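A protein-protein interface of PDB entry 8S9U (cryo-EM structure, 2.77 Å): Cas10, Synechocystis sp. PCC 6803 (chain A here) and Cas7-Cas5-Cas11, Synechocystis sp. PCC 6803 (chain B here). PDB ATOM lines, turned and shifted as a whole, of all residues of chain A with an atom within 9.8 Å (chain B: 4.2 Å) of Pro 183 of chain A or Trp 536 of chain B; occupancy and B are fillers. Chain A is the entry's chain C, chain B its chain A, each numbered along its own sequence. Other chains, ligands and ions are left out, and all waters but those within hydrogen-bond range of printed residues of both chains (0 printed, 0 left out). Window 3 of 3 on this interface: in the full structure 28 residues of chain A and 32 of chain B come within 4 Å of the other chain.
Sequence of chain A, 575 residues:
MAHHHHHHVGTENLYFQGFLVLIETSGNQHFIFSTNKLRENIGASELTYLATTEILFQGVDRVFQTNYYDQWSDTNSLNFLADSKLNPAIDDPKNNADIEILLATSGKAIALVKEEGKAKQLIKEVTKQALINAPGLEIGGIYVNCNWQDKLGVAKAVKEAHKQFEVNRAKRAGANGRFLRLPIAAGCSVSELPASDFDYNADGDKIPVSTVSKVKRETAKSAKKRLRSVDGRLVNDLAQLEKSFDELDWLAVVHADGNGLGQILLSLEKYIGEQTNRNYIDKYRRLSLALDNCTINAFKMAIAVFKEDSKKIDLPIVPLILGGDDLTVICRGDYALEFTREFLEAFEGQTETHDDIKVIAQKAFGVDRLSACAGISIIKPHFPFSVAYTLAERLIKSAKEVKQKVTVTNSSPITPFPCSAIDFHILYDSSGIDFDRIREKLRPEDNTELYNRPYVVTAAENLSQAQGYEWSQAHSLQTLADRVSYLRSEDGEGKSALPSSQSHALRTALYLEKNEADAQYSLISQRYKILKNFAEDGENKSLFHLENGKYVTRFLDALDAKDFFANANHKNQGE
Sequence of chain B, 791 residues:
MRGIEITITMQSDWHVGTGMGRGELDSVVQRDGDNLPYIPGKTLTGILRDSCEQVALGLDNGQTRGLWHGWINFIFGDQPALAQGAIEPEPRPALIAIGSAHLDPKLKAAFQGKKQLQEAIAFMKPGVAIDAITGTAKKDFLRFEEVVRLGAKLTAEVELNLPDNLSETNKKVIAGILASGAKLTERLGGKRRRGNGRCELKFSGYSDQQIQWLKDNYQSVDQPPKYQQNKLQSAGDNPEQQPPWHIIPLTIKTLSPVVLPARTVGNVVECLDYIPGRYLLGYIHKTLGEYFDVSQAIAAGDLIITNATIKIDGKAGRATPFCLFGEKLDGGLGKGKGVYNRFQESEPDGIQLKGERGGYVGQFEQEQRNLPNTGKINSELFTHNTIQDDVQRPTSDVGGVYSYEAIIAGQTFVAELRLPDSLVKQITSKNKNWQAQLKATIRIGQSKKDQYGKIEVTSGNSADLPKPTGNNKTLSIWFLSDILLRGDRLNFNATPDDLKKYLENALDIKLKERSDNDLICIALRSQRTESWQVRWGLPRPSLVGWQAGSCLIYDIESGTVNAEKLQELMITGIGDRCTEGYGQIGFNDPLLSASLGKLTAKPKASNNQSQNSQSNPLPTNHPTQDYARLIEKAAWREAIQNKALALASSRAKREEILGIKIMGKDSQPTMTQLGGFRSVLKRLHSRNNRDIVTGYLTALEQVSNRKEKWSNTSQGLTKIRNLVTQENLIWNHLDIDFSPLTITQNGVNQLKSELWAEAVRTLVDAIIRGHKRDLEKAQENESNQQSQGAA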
ATOM      1  N   LEU A 180      11.296  22.745  38.818  1.00  0.00           N
ATOM      2  CA  LEU A 180      10.231  22.517  37.860  1.00  0.00           C
ATOM      3  C   LEU A 180      10.456  23.369  36.629  1.00  0.00           C
ATOM      4  O   LEU A 180      10.816  24.542  36.719  1.00  0.00           O
ATOM      5  CB  LEU A 180       8.870  22.826  38.472  1.00  0.00           C
ATOM      6  CG  LEU A 180       8.153  21.658  39.141  1.00  0.00           C
ATOM      7  CD1 LEU A 180       8.839  21.281  40.408  1.00  0.00           C
ATOM      8  CD2 LEU A 180       6.720  22.020  39.415  1.00  0.00           C
ATOM      9  N   ARG A 181      10.248  22.762  35.475  1.00  0.00           N
ATOM     10  CA  ARG A 181      10.416  23.463  34.219  1.00  0.00           C
ATOM     11  C   ARG A 181       9.329  24.496  33.988  1.00  0.00           C
ATOM     12  O   ARG A 181       8.168  24.307  34.355  1.00  0.00           O
ATOM     13  CB  ARG A 181      10.435  22.471  33.061  1.00  0.00           C
ATOM     14  CG  ARG A 181      10.614  23.108  31.699  1.00  0.00           C
ATOM     15  CD  ARG A 181      12.057  23.318  31.347  1.00  0.00           C
ATOM     16  NE  ARG A 181      12.628  22.199  30.626  1.00  0.00           N
ATOM     17  CZ  ARG A 181      13.082  22.282  29.388  1.00  0.00           C
ATOM     18  NH1 ARG A 181      13.033  23.432  28.754  1.00  0.00           N
ATOM     19  NH2 ARG A 181      13.596  21.223  28.790  1.00  0.00           N
ATOM     20  N   LEU A 182       9.730  25.597  33.409  1.00  0.00           N
ATOM     21  CA  LEU A 182       8.928  26.679  32.914  1.00  0.00           C
ATOM     22  C   LEU A 182       9.040  26.620  31.407  1.00  0.00           C
ATOM     23  O   LEU A 182      10.059  26.164  30.887  1.00  0.00           O
ATOM     24  CB  LEU A 182       9.399  28.049  33.403  1.00  0.00           C
ATOM     25  CG  LEU A 182       9.289  28.315  34.894  1.00  0.00           C
ATOM     26  CD1 LEU A 182       9.925  29.622  35.206  1.00  0.00           C
ATOM     27  CD2 LEU A 182       7.840  28.344  35.302  1.00  0.00           C
ATOM     28  N   PRO A 183       8.026  27.031  30.666  1.00  0.00           N
ATOM     29  CA  PRO A 183       8.127  26.889  29.213  1.00  0.00           C
ATOM     30  C   PRO A 183       9.292  27.659  28.625  1.00  0.00           C
ATOM     31  O   PRO A 183       9.965  27.164  27.716  1.00  0.00           O
ATOM     32  CB  PRO A 183       6.775  27.424  28.744  1.00  0.00           C
ATOM     33  CG  PRO A 183       5.878  27.093  29.870  1.00  0.00           C
ATOM     34  CD  PRO A 183       6.675  27.433  31.072  1.00  0.00           C
ATOM     35  N   ILE A 184       9.562  28.859  29.142  1.00  0.00           N
ATOM     36  CA  ILE A 184      10.658  29.692  28.659  1.00  0.00           C
ATOM     37  C   ILE A 184      12.041  29.270  29.124  1.00  0.00           C
ATOM     38  O   ILE A 184      13.030  29.785  28.599  1.00  0.00           O
ATOM     39  CB  ILE A 184      10.392  31.144  29.083  1.00  0.00           C
ATOM     40  CG1 ILE A 184      10.256  31.230  30.596  1.00  0.00           C
ATOM     41  CG2 ILE A 184       9.133  31.643  28.426  1.00  0.00           C
ATOM     42  CD1 ILE A 184      10.149  32.629  31.101  1.00  0.00           C
ATOM     43  N   ALA A 185      12.155  28.366  30.086  1.00  0.00           N
ATOM     44  CA  ALA A 185      13.467  27.885  30.496  1.00  0.00           C
ATOM     45  C   ALA A 185      14.047  26.918  29.477  1.00  0.00           C
ATOM     46  O   ALA A 185      13.327  26.183  28.803  1.00  0.00           O
ATOM     47  CB  ALA A 185      13.399  27.212  31.862  1.00  0.00           C
ATOM     48  N   ALA A 186      15.369  26.921  29.378  1.00  0.00           N
ATOM     49  CA  ALA A 186      16.056  26.080  28.420  1.00  0.00           C
ATOM     50  C   ALA A 186      16.253  24.700  29.013  1.00  0.00           C
ATOM     51  O   ALA A 186      16.089  24.483  30.213  1.00  0.00           O
ATOM     52  CB  ALA A 186      17.399  26.678  28.029  1.00  0.00           C
ATOM     53  N   GLY A 187      16.637  23.755  28.169  1.00  0.00           N
ATOM     54  CA  GLY A 187      16.772  22.380  28.587  1.00  0.00           C
ATOM     55  C   GLY A 187      18.223  22.006  28.815  1.00  0.00           C
ATOM     56  O   GLY A 187      19.112  22.446  28.090  1.00  0.00           O
ATOM     57  N   PRO A 194      15.374  21.562  33.546  1.00  0.00           N
ATOM     58  CA  PRO A 194      15.744  22.802  32.867  1.00  0.00           C
ATOM     59  C   PRO A 194      17.211  23.116  33.095  1.00  0.00           C
ATOM     60  O   PRO A 194      17.823  22.677  34.069  1.00  0.00           O
ATOM     61  CB  PRO A 194      14.843  23.840  33.531  1.00  0.00           C
ATOM     62  CG  PRO A 194      14.649  23.324  34.879  1.00  0.00           C
ATOM     63  CD  PRO A 194      14.531  21.839  34.721  1.00  0.00           C
ATOM     64  N   ALA A 195      17.774  23.903  32.188  1.00  0.00           N
ATOM     65  CA  ALA A 195      19.124  24.399  32.386  1.00  0.00           C
ATOM     66  C   ALA A 195      19.137  25.551  33.371  1.00  0.00           C
ATOM     67  O   ALA A 195      18.221  26.371  33.406  1.00  0.00           O
ATOM     68  CB  ALA A 195      19.730  24.851  31.066  1.00  0.00           C
ATOM     69  N   GLN B 533       4.691  21.263  24.198  1.00  0.00           N
ATOM     70  CA  GLN B 533       3.414  21.657  23.629  1.00  0.00           C
ATOM     71  C   GLN B 533       3.639  22.161  22.221  1.00  0.00           C
ATOM     72  O   GLN B 533       4.294  23.183  22.020  1.00  0.00           O
ATOM     73  CB  GLN B 533       2.694  22.710  24.447  1.00  0.00           C
ATOM     74  CG  GLN B 533       1.484  23.165  23.686  1.00  0.00           C
ATOM     75  CD  GLN B 533       0.346  23.457  24.561  1.00  0.00           C
ATOM     76  OE1 GLN B 533       0.446  23.328  25.767  1.00  0.00           O
ATOM     77  NE2 GLN B 533      -0.765  23.847  23.974  1.00  0.00           N
ATOM     78  N   VAL B 534       3.099  21.431  21.249  1.00  0.00           N
ATOM     79  CA  VAL B 534       3.343  21.725  19.848  1.00  0.00           C
ATOM     80  C   VAL B 534       2.708  23.046  19.450  1.00  0.00           C
ATOM     81  O   VAL B 534       3.187  23.717  18.531  1.00  0.00           O
ATOM     82  CB  VAL B 534       2.842  20.553  19.003  1.00  0.00           C
ATOM     83  CG1 VAL B 534       3.087  20.799  17.557  1.00  0.00           C
ATOM     84  CG2 VAL B 534       3.540  19.302  19.443  1.00  0.00           C
ATOM     85  N   ARG B 535       1.645  23.459  20.132  1.00  0.00           N
ATOM     86  CA  ARG B 535       0.985  24.706  19.782  1.00  0.00           C
ATOM     87  C   ARG B 535       1.694  25.903  20.377  1.00  0.00           C
ATOM     88  O   ARG B 535       1.512  27.020  19.894  1.00  0.00           O
ATOM     89  CB  ARG B 535      -0.466  24.697  20.242  1.00  0.00           C
ATOM     90  CG  ARG B 535      -1.269  23.550  19.704  1.00  0.00           C
ATOM     91  CD  ARG B 535      -2.740  23.780  19.904  1.00  0.00           C
ATOM     92  NE  ARG B 535      -3.513  22.614  19.519  1.00  0.00           N
ATOM     93  CZ  ARG B 535      -3.861  22.325  18.276  1.00  0.00           C
ATOM     94  NH1 ARG B 535      -3.514  23.125  17.286  1.00  0.00           N
ATOM     95  NH2 ARG B 535      -4.562  21.237  18.022  1.00  0.00           N
ATOM     96  N   TRP B 536       2.511  25.685  21.396  1.00  0.00           N
ATOM     97  CA  TRP B 536       3.280  26.738  22.030  1.00  0.00           C
ATOM     98  C   TRP B 536       4.662  26.877  21.433  1.00  0.00           C
ATOM     99  O   TRP B 536       5.257  27.954  21.522  1.00  0.00           O
ATOM    100  CB  TRP B 536       3.468  26.456  23.521  1.00  0.00           C
ATOM    101  CG  TRP B 536       2.283  26.585  24.374  1.00  0.00           C
ATOM    102  CD1 TRP B 536       1.023  26.852  23.983  1.00  0.00           C
ATOM    103  CD2 TRP B 536       2.249  26.471  25.796  1.00  0.00           C
ATOM    104  NE1 TRP B 536       0.192  26.911  25.068  1.00  0.00           N
ATOM    105  CE2 TRP B 536       0.926  26.680  26.197  1.00  0.00           C
ATOM    106  CE3 TRP B 536       3.211  26.207  26.767  1.00  0.00           C
ATOM    107  CZ2 TRP B 536       0.540  26.635  27.522  1.00  0.00           C
ATOM    108  CZ3 TRP B 536       2.825  26.166  28.075  1.00  0.00           C
ATOM    109  CH2 TRP B 536       1.504  26.376  28.443  1.00  0.00           C
ATOM    110  N   GLY B 537       5.175  25.821  20.815  1.00  0.00           N
ATOM    111  CA  GLY B 537       6.555  25.800  20.388  1.00  0.00           C
ATOM    112  C   GLY B 537       7.502  25.889  21.555  1.00  0.00           C
ATOM    113  O   GLY B 537       8.646  26.317  21.396  1.00  0.00           O
ATOM    114  N   LEU B 538       7.050  25.475  22.728  1.00  0.00           N
ATOM    115  CA  LEU B 538       7.789  25.534  23.974  1.00  0.00           C
ATOM    116  C   LEU B 538       7.405  24.307  24.773  1.00  0.00           C
ATOM    117  O   LEU B 538       6.332  23.738  24.558  1.00  0.00           O
ATOM    118  CB  LEU B 538       7.455  26.800  24.767  1.00  0.00           C
ATOM    119  CG  LEU B 538       7.940  28.124  24.204  1.00  0.00           C
ATOM    120  CD1 LEU B 538       7.421  29.235  25.060  1.00  0.00           C
ATOM    121  CD2 LEU B 538       9.434  28.134  24.181  1.00  0.00           C
ATOM    122  N   PRO B 539       8.257  23.861  25.685  1.00  0.00           N
ATOM    123  CA  PRO B 539       7.852  22.778  26.572  1.00  0.00           C
ATOM    124  C   PRO B 539       6.678  23.199  27.429  1.00  0.00           C
ATOM    125  O   PRO B 539       6.498  24.377  27.738  1.00  0.00           O
ATOM    126  CB  PRO B 539       9.108  22.512  27.397  1.00  0.00           C
ATOM    127  CG  PRO B 539       9.806  23.749  27.390  1.00  0.00           C
ATOM    128  CD  PRO B 539       9.579  24.375  26.062  1.00  0.00           C
ATOM    129  N   PRO B 541       4.806  23.282  31.082  1.00  0.00           N
ATOM    130  CA  PRO B 541       5.434  23.366  32.392  1.00  0.00           C
ATOM    131  C   PRO B 541       5.727  21.957  32.850  1.00  0.00           C
ATOM    132  O   PRO B 541       5.500  21.007  32.100  1.00  0.00           O
ATOM    133  CB  PRO B 541       4.361  24.048  33.245  1.00  0.00           C
ATOM    134  CG  PRO B 541       3.114  23.826  32.471  1.00  0.00           C
ATOM    135  CD  PRO B 541       3.558  24.049  31.089  1.00  0.00           C
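The side-chain amide nitrogen (NE2) of Gln 533 of chain B lies close to the indole nitrogen (NE1) of Trp 536 of chain B, 3.4 Å away. O of Leu 538 of chain B sits at hydrogen-bond distance from N of Gln 533 of chain B, 3.0 Å away. NH1 of Arg 181 of chain A lies within hydrogen-bond range of O of Ala 185 of chain A (2.8 Å).
Of the 8 printed residues of chain B, 4 touch a printed residue of chain A. Hydrophobic or aromatic side chains of chain B that line the printed part of chain A: Trp 536, Leu 538, Pro 539 and Pro 541. Hydrophobic or aromatic side chains of chain A within 4 Å of the printed part of chain B: Pro 183.
Printed residues of chain B within 4 Å of Pro 183 of chain A: Trp 536, Leu 538 and Pro 539. Trp 536 of chain B touches one residue of chain A. No residue of chain A comes within 4 Å of Gln 533 of chain B. Of chain A, only Pro 183 comes within 4 Å of Leu 538 of chain B. Pro 539 of chain B touches just these residues of chain A: Arg 181 and Pro 183. Of the printed residues of chain B, Arg 181 of chain A touches Pro 539 and Pro 541. Of the printed residues of chain A, Pro 541 of chain B touches Arg 181. Leu 182 of chain A touches none of the printed residues of chain B. Leu 180 of chain A touches none of the printed residues of chain B. The nearest printed residue of chain B that does not touch Arg 181 of chain A is Leu 538 of chain B (6.9 Å).
Pro 539 of chain B touches Arg 181 of chain A. Pro 541 of chain B touches Arg 181 of chain A (CA to O, 3.5 Å). Trp 536 of chain B touches Pro 183 of chain A. Leu 538 of chain B touches Pro 183 of chain A (CD2 to O, 3.7 Å). Pro 183 of chain A touches Pro 539 of chain B (CB to O, 3.2 Å).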
